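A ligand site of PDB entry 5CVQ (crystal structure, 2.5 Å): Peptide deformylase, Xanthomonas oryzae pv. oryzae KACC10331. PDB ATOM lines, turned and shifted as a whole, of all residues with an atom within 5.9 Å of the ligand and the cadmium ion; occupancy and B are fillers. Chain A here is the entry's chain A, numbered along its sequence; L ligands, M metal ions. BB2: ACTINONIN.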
ATOM      1  N   ALA A  42      29.602 -13.765  10.999  1.00  0.00           N
ATOM      2  CA  ALA A  42      28.321 -14.300  11.424  1.00  0.00           C
ATOM      3  C   ALA A  42      28.062 -13.870  12.879  1.00  0.00           C
ATOM      4  O   ALA A  42      27.024 -14.204  13.432  1.00  0.00           O
ATOM      5  CB  ALA A  42      28.261 -15.850  11.279  1.00  0.00           C
ATOM      6  N   HIS A  43      28.995 -13.144  13.467  1.00  0.00           N
ATOM      7  CA  HIS A  43      28.903 -12.660  14.865  1.00  0.00           C
ATOM      8  C   HIS A  43      28.818 -13.776  15.881  1.00  0.00           C
ATOM      9  O   HIS A  43      28.115 -13.651  16.874  1.00  0.00           O
ATOM     10  CB  HIS A  43      27.734 -11.674  15.056  1.00  0.00           C
ATOM     11  CG  HIS A  43      27.834 -10.441  14.204  1.00  0.00           C
ATOM     12  ND1 HIS A  43      27.459  -9.190  14.636  1.00  0.00           N
ATOM     13  CD2 HIS A  43      28.314 -10.261  12.948  1.00  0.00           C
ATOM     14  CE1 HIS A  43      27.669  -8.298  13.685  1.00  0.00           C
ATOM     15  NE2 HIS A  43      28.200  -8.922  12.652  1.00  0.00           N
ATOM     16  N   GLY A  44      29.512 -14.881  15.652  1.00  0.00           N
ATOM     17  CA  GLY A  44      29.499 -15.955  16.642  1.00  0.00           C
ATOM     18  C   GLY A  44      30.609 -15.852  17.662  1.00  0.00           C
ATOM     19  O   GLY A  44      31.520 -15.048  17.504  1.00  0.00           O
ATOM     20  N   VAL A  45      30.547 -16.684  18.713  1.00  0.00           N
ATOM     21  CA  VAL A  45      31.654 -16.727  19.688  1.00  0.00           C
ATOM     22  C   VAL A  45      32.404 -18.067  19.511  1.00  0.00           C
ATOM     23  O   VAL A  45      33.449 -18.360  20.169  1.00  0.00           O
ATOM     24  CB  VAL A  45      31.158 -16.528  21.162  1.00  0.00           C
ATOM     25  CG1 VAL A  45      30.489 -15.151  21.293  1.00  0.00           C
ATOM     26  CG2 VAL A  45      30.188 -17.632  21.583  1.00  0.00           C
ATOM     27  N   GLY A  46      31.891 -18.886  18.628  1.00  0.00           N
ATOM     28  CA  GLY A  46      32.543 -20.155  18.393  1.00  0.00           C
ATOM     29  C   GLY A  46      32.133 -20.495  16.996  1.00  0.00           C
ATOM     30  O   GLY A  46      31.123 -19.947  16.493  1.00  0.00           O
ATOM     31  N   LEU A  47      32.925 -21.359  16.362  1.00  0.00           N
ATOM     32  CA  LEU A  47      32.563 -21.967  15.101  1.00  0.00           C
ATOM     33  C   LEU A  47      33.274 -23.326  14.991  1.00  0.00           C
ATOM     34  O   LEU A  47      34.455 -23.467  15.371  1.00  0.00           O
ATOM     35  CB  LEU A  47      32.937 -21.078  13.938  1.00  0.00           C
ATOM     36  CG  LEU A  47      32.483 -21.576  12.572  1.00  0.00           C
ATOM     37  CD1 LEU A  47      30.979 -21.394  12.325  1.00  0.00           C
ATOM     38  CD2 LEU A  47      33.274 -20.842  11.515  1.00  0.00           C
ATOM     39  N   ALA A  48      32.536 -24.317  14.485  1.00  0.00           N
ATOM     40  CA  ALA A  48      33.023 -25.655  14.350  1.00  0.00           C
ATOM     41  C   ALA A  48      33.178 -25.988  12.867  1.00  0.00           C
ATOM     42  O   ALA A  48      32.313 -25.629  12.061  1.00  0.00           O
ATOM     43  CB  ALA A  48      32.065 -26.630  15.038  1.00  0.00           C
ATOM     44  N   GLN A  51      30.299 -26.958  10.536  1.00  0.00           N
ATOM     45  CA  GLN A  51      29.326 -25.928  10.203  1.00  0.00           C
ATOM     46  C   GLN A  51      29.583 -25.278   8.857  1.00  0.00           C
ATOM     47  O   GLN A  51      28.725 -24.572   8.325  1.00  0.00           O
ATOM     48  CB  GLN A  51      29.284 -24.882  11.288  1.00  0.00           C
ATOM     49  CG  GLN A  51      28.639 -25.370  12.568  1.00  0.00           C
ATOM     50  CD  GLN A  51      28.684 -24.271  13.610  1.00  0.00           C
ATOM     51  OE1 GLN A  51      29.725 -24.023  14.247  1.00  0.00           O
ATOM     52  NE2 GLN A  51      27.599 -23.546  13.746  1.00  0.00           N
ATOM     53  N   TRP A  96      21.652 -19.521  28.127  1.00  0.00           N
ATOM     54  CA  TRP A  96      21.130 -19.372  26.785  1.00  0.00           C
ATOM     55  C   TRP A  96      22.180 -19.725  25.737  1.00  0.00           C
ATOM     56  O   TRP A  96      23.391 -19.375  25.857  1.00  0.00           O
ATOM     57  CB  TRP A  96      20.667 -17.945  26.567  1.00  0.00           C
ATOM     58  CG  TRP A  96      19.445 -17.632  27.339  1.00  0.00           C
ATOM     59  CD1 TRP A  96      19.361 -16.906  28.512  1.00  0.00           C
ATOM     60  CD2 TRP A  96      18.099 -18.042  27.011  1.00  0.00           C
ATOM     61  NE1 TRP A  96      18.061 -16.838  28.912  1.00  0.00           N
ATOM     62  CE2 TRP A  96      17.255 -17.516  28.018  1.00  0.00           C
ATOM     63  CE3 TRP A  96      17.533 -18.775  25.952  1.00  0.00           C
ATOM     64  CZ2 TRP A  96      15.874 -17.723  28.011  1.00  0.00           C
ATOM     65  CZ3 TRP A  96      16.161 -18.988  25.954  1.00  0.00           C
ATOM     66  CH2 TRP A  96      15.349 -18.476  26.976  1.00  0.00           C
ATOM     67  N   GLU A  97      21.700 -20.370  24.675  1.00  0.00           N
ATOM     68  CA  GLU A  97      22.508 -20.667  23.488  1.00  0.00           C
ATOM     69  C   GLU A  97      21.720 -20.452  22.217  1.00  0.00           C
ATOM     70  O   GLU A  97      20.484 -20.628  22.203  1.00  0.00           O
ATOM     71  CB  GLU A  97      23.005 -22.103  23.575  1.00  0.00           C
ATOM     72  CG  GLU A  97      23.962 -22.344  24.745  1.00  0.00           C
ATOM     73  CD  GLU A  97      24.589 -23.712  24.670  1.00  0.00           C
ATOM     74  OE1 GLU A  97      24.679 -24.305  23.541  1.00  0.00           O
ATOM     75  OE2 GLU A  97      24.970 -24.215  25.758  1.00  0.00           O
ATOM     76  N   GLY A  98      22.415 -20.050  21.157  1.00  0.00           N
ATOM     77  CA  GLY A  98      21.857 -20.123  19.804  1.00  0.00           C
ATOM     78  C   GLY A  98      22.928 -20.679  18.889  1.00  0.00           C
ATOM     79  O   GLY A  98      24.121 -20.631  19.210  1.00  0.00           O
ATOM     80  N   CYS A  99      22.546 -21.185  17.744  1.00  0.00           N
ATOM     81  CA  CYS A  99      23.506 -21.853  16.896  1.00  0.00           C
ATOM     82  C   CYS A  99      23.350 -21.145  15.577  1.00  0.00           C
ATOM     83  O   CYS A  99      22.223 -20.975  15.142  1.00  0.00           O
ATOM     84  CB  CYS A  99      23.191 -23.377  16.821  1.00  0.00           C
ATOM     85  SG  CYS A  99      24.154 -24.485  15.745  1.00  0.00           S
ATOM     86  N   LEU A 100      24.463 -20.738  14.971  1.00  0.00           N
ATOM     87  CA  LEU A 100      24.500 -20.162  13.628  1.00  0.00           C
ATOM     88  C   LEU A 100      23.985 -21.145  12.543  1.00  0.00           C
ATOM     89  O   LEU A 100      23.602 -20.730  11.431  1.00  0.00           O
ATOM     90  CB  LEU A 100      25.923 -19.758  13.238  1.00  0.00           C
ATOM     91  CG  LEU A 100      26.586 -18.805  14.185  1.00  0.00           C
ATOM     92  CD1 LEU A 100      28.087 -18.779  13.927  1.00  0.00           C
ATOM     93  CD2 LEU A 100      25.918 -17.456  13.995  1.00  0.00           C
ATOM     94  N   SER A 101      24.007 -22.442  12.855  1.00  0.00           N
ATOM     95  CA  SER A 101      23.313 -23.375  11.989  1.00  0.00           C
ATOM     96  C   SER A 101      21.746 -23.368  12.224  1.00  0.00           C
ATOM     97  O   SER A 101      20.988 -23.962  11.485  1.00  0.00           O
ATOM     98  CB  SER A 101      23.996 -24.776  12.074  1.00  0.00           C
ATOM     99  OG  SER A 101      25.327 -24.694  11.588  1.00  0.00           O
ATOM    100  N   LEU A 105      16.953 -18.916  16.486  1.00  0.00           N
ATOM    101  CA  LEU A 105      16.458 -19.604  17.693  1.00  0.00           C
ATOM    102  C   LEU A 105      17.382 -19.525  18.909  1.00  0.00           C
ATOM    103  O   LEU A 105      18.585 -19.391  18.753  1.00  0.00           O
ATOM    104  CB  LEU A 105      16.001 -21.050  17.355  1.00  0.00           C
ATOM    105  CG  LEU A 105      14.747 -21.027  16.447  1.00  0.00           C
ATOM    106  CD1 LEU A 105      14.634 -22.328  15.720  1.00  0.00           C
ATOM    107  CD2 LEU A 105      13.429 -20.723  17.190  1.00  0.00           C
ATOM    108  N   ARG A 106      16.811 -19.626  20.116  1.00  0.00           N
ATOM    109  CA  ARG A 106      17.574 -19.781  21.349  1.00  0.00           C
ATOM    110  C   ARG A 106      16.841 -20.818  22.230  1.00  0.00           C
ATOM    111  O   ARG A 106      15.652 -20.986  22.061  1.00  0.00           O
ATOM    112  CB  ARG A 106      17.655 -18.476  22.141  1.00  0.00           C
ATOM    113  CG  ARG A 106      17.964 -17.219  21.397  1.00  0.00           C
ATOM    114  CD  ARG A 106      19.463 -16.970  21.302  1.00  0.00           C
ATOM    115  NE  ARG A 106      19.756 -15.781  20.494  1.00  0.00           N
ATOM    116  CZ  ARG A 106      19.985 -15.769  19.178  1.00  0.00           C
ATOM    117  NH1 ARG A 106      20.187 -14.625  18.591  1.00  0.00           N
ATOM    118  NH2 ARG A 106      20.008 -16.895  18.457  1.00  0.00           N
ATOM    119  N   PHE A 134      30.913 -19.612  31.001  1.00  0.00           N
ATOM    120  CA  PHE A 134      30.718 -19.330  29.575  1.00  0.00           C
ATOM    121  C   PHE A 134      31.781 -19.931  28.653  1.00  0.00           C
ATOM    122  O   PHE A 134      31.463 -20.600  27.643  1.00  0.00           O
ATOM    123  CB  PHE A 134      30.553 -17.830  29.309  1.00  0.00           C
ATOM    124  CG  PHE A 134      30.048 -17.522  27.952  1.00  0.00           C
ATOM    125  CD1 PHE A 134      28.769 -17.964  27.544  1.00  0.00           C
ATOM    126  CD2 PHE A 134      30.829 -16.794  27.039  1.00  0.00           C
ATOM    127  CE1 PHE A 134      28.299 -17.663  26.254  1.00  0.00           C
ATOM    128  CE2 PHE A 134      30.353 -16.509  25.746  1.00  0.00           C
ATOM    129  CZ  PHE A 134      29.101 -16.959  25.360  1.00  0.00           C
ATOM    130  N   ARG A 137      31.118 -23.423  28.285  1.00  0.00           N
ATOM    131  CA  ARG A 137      29.912 -23.675  27.488  1.00  0.00           C
ATOM    132  C   ARG A 137      30.211 -23.668  25.956  1.00  0.00           C
ATOM    133  O   ARG A 137      29.745 -24.528  25.164  1.00  0.00           O
ATOM    134  CB  ARG A 137      28.853 -22.604  27.808  1.00  0.00           C
ATOM    135  CG  ARG A 137      27.566 -22.679  26.983  1.00  0.00           C
ATOM    136  CD  ARG A 137      26.550 -21.653  27.510  1.00  0.00           C
ATOM    137  NE  ARG A 137      26.285 -21.897  28.925  1.00  0.00           N
ATOM    138  CZ  ARG A 137      25.384 -22.771  29.382  1.00  0.00           C
ATOM    139  NH1 ARG A 137      24.574 -23.399  28.529  1.00  0.00           N
ATOM    140  NH2 ARG A 137      25.282 -22.991  30.706  1.00  0.00           N
ATOM    141  N   VAL A 138      30.983 -22.662  25.557  1.00  0.00           N
ATOM    142  CA  VAL A 138      31.337 -22.468  24.177  1.00  0.00           C
ATOM    143  C   VAL A 138      32.042 -23.696  23.673  1.00  0.00           C
ATOM    144  O   VAL A 138      31.663 -24.218  22.600  1.00  0.00           O
ATOM    145  CB  VAL A 138      32.169 -21.209  23.962  1.00  0.00           C
ATOM    146  CG1 VAL A 138      32.620 -21.111  22.490  1.00  0.00           C
ATOM    147  CG2 VAL A 138      31.330 -19.986  24.382  1.00  0.00           C
ATOM    148  N   HIS A 141      29.662 -26.764  23.434  1.00  0.00           N
ATOM    149  CA  HIS A 141      28.843 -26.507  22.224  1.00  0.00           C
ATOM    150  C   HIS A 141      29.594 -26.853  20.920  1.00  0.00           C
ATOM    151  O   HIS A 141      29.038 -27.544  20.030  1.00  0.00           O
ATOM    152  CB  HIS A 141      28.373 -25.043  22.199  1.00  0.00           C
ATOM    153  CG  HIS A 141      27.525 -24.699  21.012  1.00  0.00           C
ATOM    154  ND1 HIS A 141      26.188 -24.349  21.126  1.00  0.00           N
ATOM    155  CD2 HIS A 141      27.820 -24.633  19.684  1.00  0.00           C
ATOM    156  CE1 HIS A 141      25.692 -24.101  19.928  1.00  0.00           C
ATOM    157  NE2 HIS A 141      26.657 -24.276  19.036  1.00  0.00           N
ATOM    158  N   GLU A 142      30.819 -26.354  20.770  1.00  0.00           N
ATOM    159  CA  GLU A 142      31.555 -26.618  19.544  1.00  0.00           C
ATOM    160  C   GLU A 142      31.922 -28.101  19.500  1.00  0.00           C
ATOM    161  O   GLU A 142      31.806 -28.736  18.441  1.00  0.00           O
ATOM    162  CB  GLU A 142      32.795 -25.720  19.396  1.00  0.00           C
ATOM    163  CG  GLU A 142      32.551 -24.221  19.521  1.00  0.00           C
ATOM    164  CD  GLU A 142      31.473 -23.761  18.553  1.00  0.00           C
ATOM    165  OE1 GLU A 142      31.247 -24.448  17.508  1.00  0.00           O
ATOM    166  OE2 GLU A 142      30.822 -22.742  18.852  1.00  0.00           O
ATOM    167  N   HIS A 145      29.191 -30.339  18.016  1.00  0.00           N
ATOM    168  CA  HIS A 145      29.257 -30.352  16.517  1.00  0.00           C
ATOM    169  C   HIS A 145      30.213 -31.393  15.956  1.00  0.00           C
ATOM    170  O   HIS A 145      29.907 -32.000  14.926  1.00  0.00           O
ATOM    171  CB  HIS A 145      29.681 -29.009  15.918  1.00  0.00           C
ATOM    172  CG  HIS A 145      28.581 -27.993  15.932  1.00  0.00           C
ATOM    173  ND1 HIS A 145      27.424 -28.152  15.211  1.00  0.00           N
ATOM    174  CD2 HIS A 145      28.468 -26.808  16.582  1.00  0.00           C
ATOM    175  CE1 HIS A 145      26.640 -27.100  15.394  1.00  0.00           C
ATOM    176  NE2 HIS A 145      27.254 -26.275  16.225  1.00  0.00           N
ATOM    177  N   LEU A 150      23.539 -31.494  18.147  1.00  0.00           N
ATOM    178  CA  LEU A 150      23.072 -30.096  18.169  1.00  0.00           C
ATOM    179  C   LEU A 150      22.340 -29.818  19.471  1.00  0.00           C
ATOM    180  O   LEU A 150      21.817 -30.757  20.120  1.00  0.00           O
ATOM    181  CB  LEU A 150      22.183 -29.814  16.956  1.00  0.00           C
ATOM    182  CG  LEU A 150      22.993 -30.079  15.670  1.00  0.00           C
ATOM    183  CD1 LEU A 150      22.161 -30.316  14.428  1.00  0.00           C
ATOM    184  CD2 LEU A 150      23.987 -28.952  15.428  1.00  0.00           C
ATOM    185  N   ASP A 164      14.713 -15.431  19.001  1.00  0.00           N
ATOM    186  CA  ASP A 164      15.468 -14.421  19.818  1.00  0.00           C
ATOM    187  C   ASP A 164      14.680 -13.151  20.037  1.00  0.00           C
ATOM    188  O   ASP A 164      14.625 -12.643  21.160  1.00  0.00           O
ATOM    189  CB  ASP A 164      16.857 -14.066  19.266  1.00  0.00           C
ATOM    190  CG  ASP A 164      17.659 -13.151  20.249  1.00  0.00           C
ATOM    191  OD1 ASP A 164      18.139 -12.075  19.831  1.00  0.00           O
ATOM    192  OD2 ASP A 164      17.843 -13.460  21.462  1.00  0.00           O
HETATM  193  C5  BB2 L   1      28.030 -20.142  17.345  1.00  0.00           C
HETATM  194  C3  BB2 L   1      27.864 -21.544  16.837  1.00  0.00           C
HETATM  195  O4  BB2 L   1      26.813 -21.877  16.299  1.00  0.00           O
HETATM  196  N1  BB2 L   1      28.939 -22.315  17.041  1.00  0.00           N
HETATM  197  O2  BB2 L   1      29.008 -23.665  16.702  1.00  0.00           O
HETATM  198  C6  BB2 L   1      27.306 -20.038  18.662  1.00  0.00           C
HETATM  199  C12 BB2 L   1      27.160 -18.562  19.006  1.00  0.00           C
HETATM  200  O13 BB2 L   1      28.087 -17.753  18.795  1.00  0.00           O
HETATM  201  C7  BB2 L   1      28.117 -20.785  19.753  1.00  0.00           C
HETATM  202  C8  BB2 L   1      27.305 -20.776  21.050  1.00  0.00           C
HETATM  203  C9  BB2 L   1      28.180 -21.047  22.230  1.00  0.00           C
HETATM  204  C10 BB2 L   1      27.288 -21.314  23.424  1.00  0.00           C
HETATM  205  C11 BB2 L   1      26.905 -20.004  24.075  1.00  0.00           C
HETATM  206  N14 BB2 L   1      25.980 -18.246  19.540  1.00  0.00           N
HETATM  207  C15 BB2 L   1      25.639 -16.984  20.198  1.00  0.00           C
HETATM  208  C16 BB2 L   1      24.775 -16.022  19.305  1.00  0.00           C
HETATM  209  C18 BB2 L   1      25.345 -15.646  17.911  1.00  0.00           C
HETATM  210  C17 BB2 L   1      23.407 -16.645  19.053  1.00  0.00           C
HETATM  211  C19 BB2 L   1      24.953 -17.302  21.535  1.00  0.00           C
HETATM  212  O20 BB2 L   1      24.266 -18.323  21.676  1.00  0.00           O
HETATM  213  N21 BB2 L   1      25.153 -16.423  22.540  1.00  0.00           N
HETATM  214  C22 BB2 L   1      24.760 -16.716  23.957  1.00  0.00           C
HETATM  215  C23 BB2 L   1      25.790 -15.100  22.378  1.00  0.00           C
HETATM  216  C24 BB2 L   1      26.117 -14.681  23.802  1.00  0.00           C
HETATM  217  C25 BB2 L   1      25.256 -15.512  24.748  1.00  0.00           C
HETATM  218  C26 BB2 L   1      23.238 -16.767  24.095  1.00  0.00           C
HETATM  219  O27 BB2 L   1      22.785 -15.475  23.784  1.00  0.00           O
HETATM  220 CD    CD M   1      26.560 -24.183  16.805  1.00  0.00          CD
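Merely in contact with the cadmium ion: Gln 51 (3.3 Å).
The nearest printed residue that does not touch the cadmium ion is Leu 100 (4.4 Å).
The cadmium ion is bound by NE2 of His 141 (2.2 Å), NE2 of His 145 (2.3 Å), O4 of the ligand (2.4 Å), O2 of the ligand (2.5 Å) and SG of Cys 99 (2.6 Å).
Merely in contact with the ligand: Gly 44, Trp 96, Glu 97, Arg 106, Phe 134, His 43, Arg 137 and Val 138.
Hydrophobic or aromatic side chains that line the ligand: Val 45, Trp 96, Leu 100, Phe 134, Val 138, His 141 and His 145.
17 residues have an atom within 4 Å of the ligand: His 43, Gly 44, Val 45, Gly 46, Gln 51, Trp 96, Glu 97, Gly 98, Cys 99, Leu 100, Arg 106, Phe 134, Arg 137, Val 138, His 141, Glu 142 and His 145.
N of Val 45 lies within hydrogen-bond range of O13 of the ligand (2.7 Å).
O of Gly 98 sits at hydrogen-bond distance from N14 of the ligand.
The backbone NH (N) of Gly 98 is in hydrogen-bond range of an oxygen (O20) of the ligand, at 2.6 Å.
A nitrogen (N1) of the ligand sits close to the backbone carbonyl oxygen (O) of Gly 46, 3.3 Å away.
The side-chain carboxylate (OE2) of Glu 142 is in hydrogen-bond range of a nitrogen (N1) of the ligand (2.6 Å).
The backbone NH of Leu 100 sits close to an oxygen (O4) of the ligand, at 2.9 Å.
The side-chain amide oxygen of Gln 51 lies within hydrogen-bond range of a nitrogen (N1) of the ligand.
OD2 of Asp 164 is in salt-bridge range of NE of Arg 106, at 3.2 Å.
The side-chain carboxylate (OE1) of Glu 142 is in hydrogen-bond range of the backbone NH (N) of Ala 48, at 3.3 Å.
OE1 of Gln 51 lies within hydrogen-bond range of N of Ala 48 (2.8 Å).
ND1 of His 141 lies within hydrogen-bond range of OE1 of Glu 97.
NE2 of Gln 51 lies within hydrogen-bond range of OG of Ser 101 (3.3 Å).
The backbone NH of Ser 101 lies close to the side-chain sulfur of Cys 99 (3.5 Å).
NH1 of Arg 137 lies within salt-bridge range of OE2 of Glu 97.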
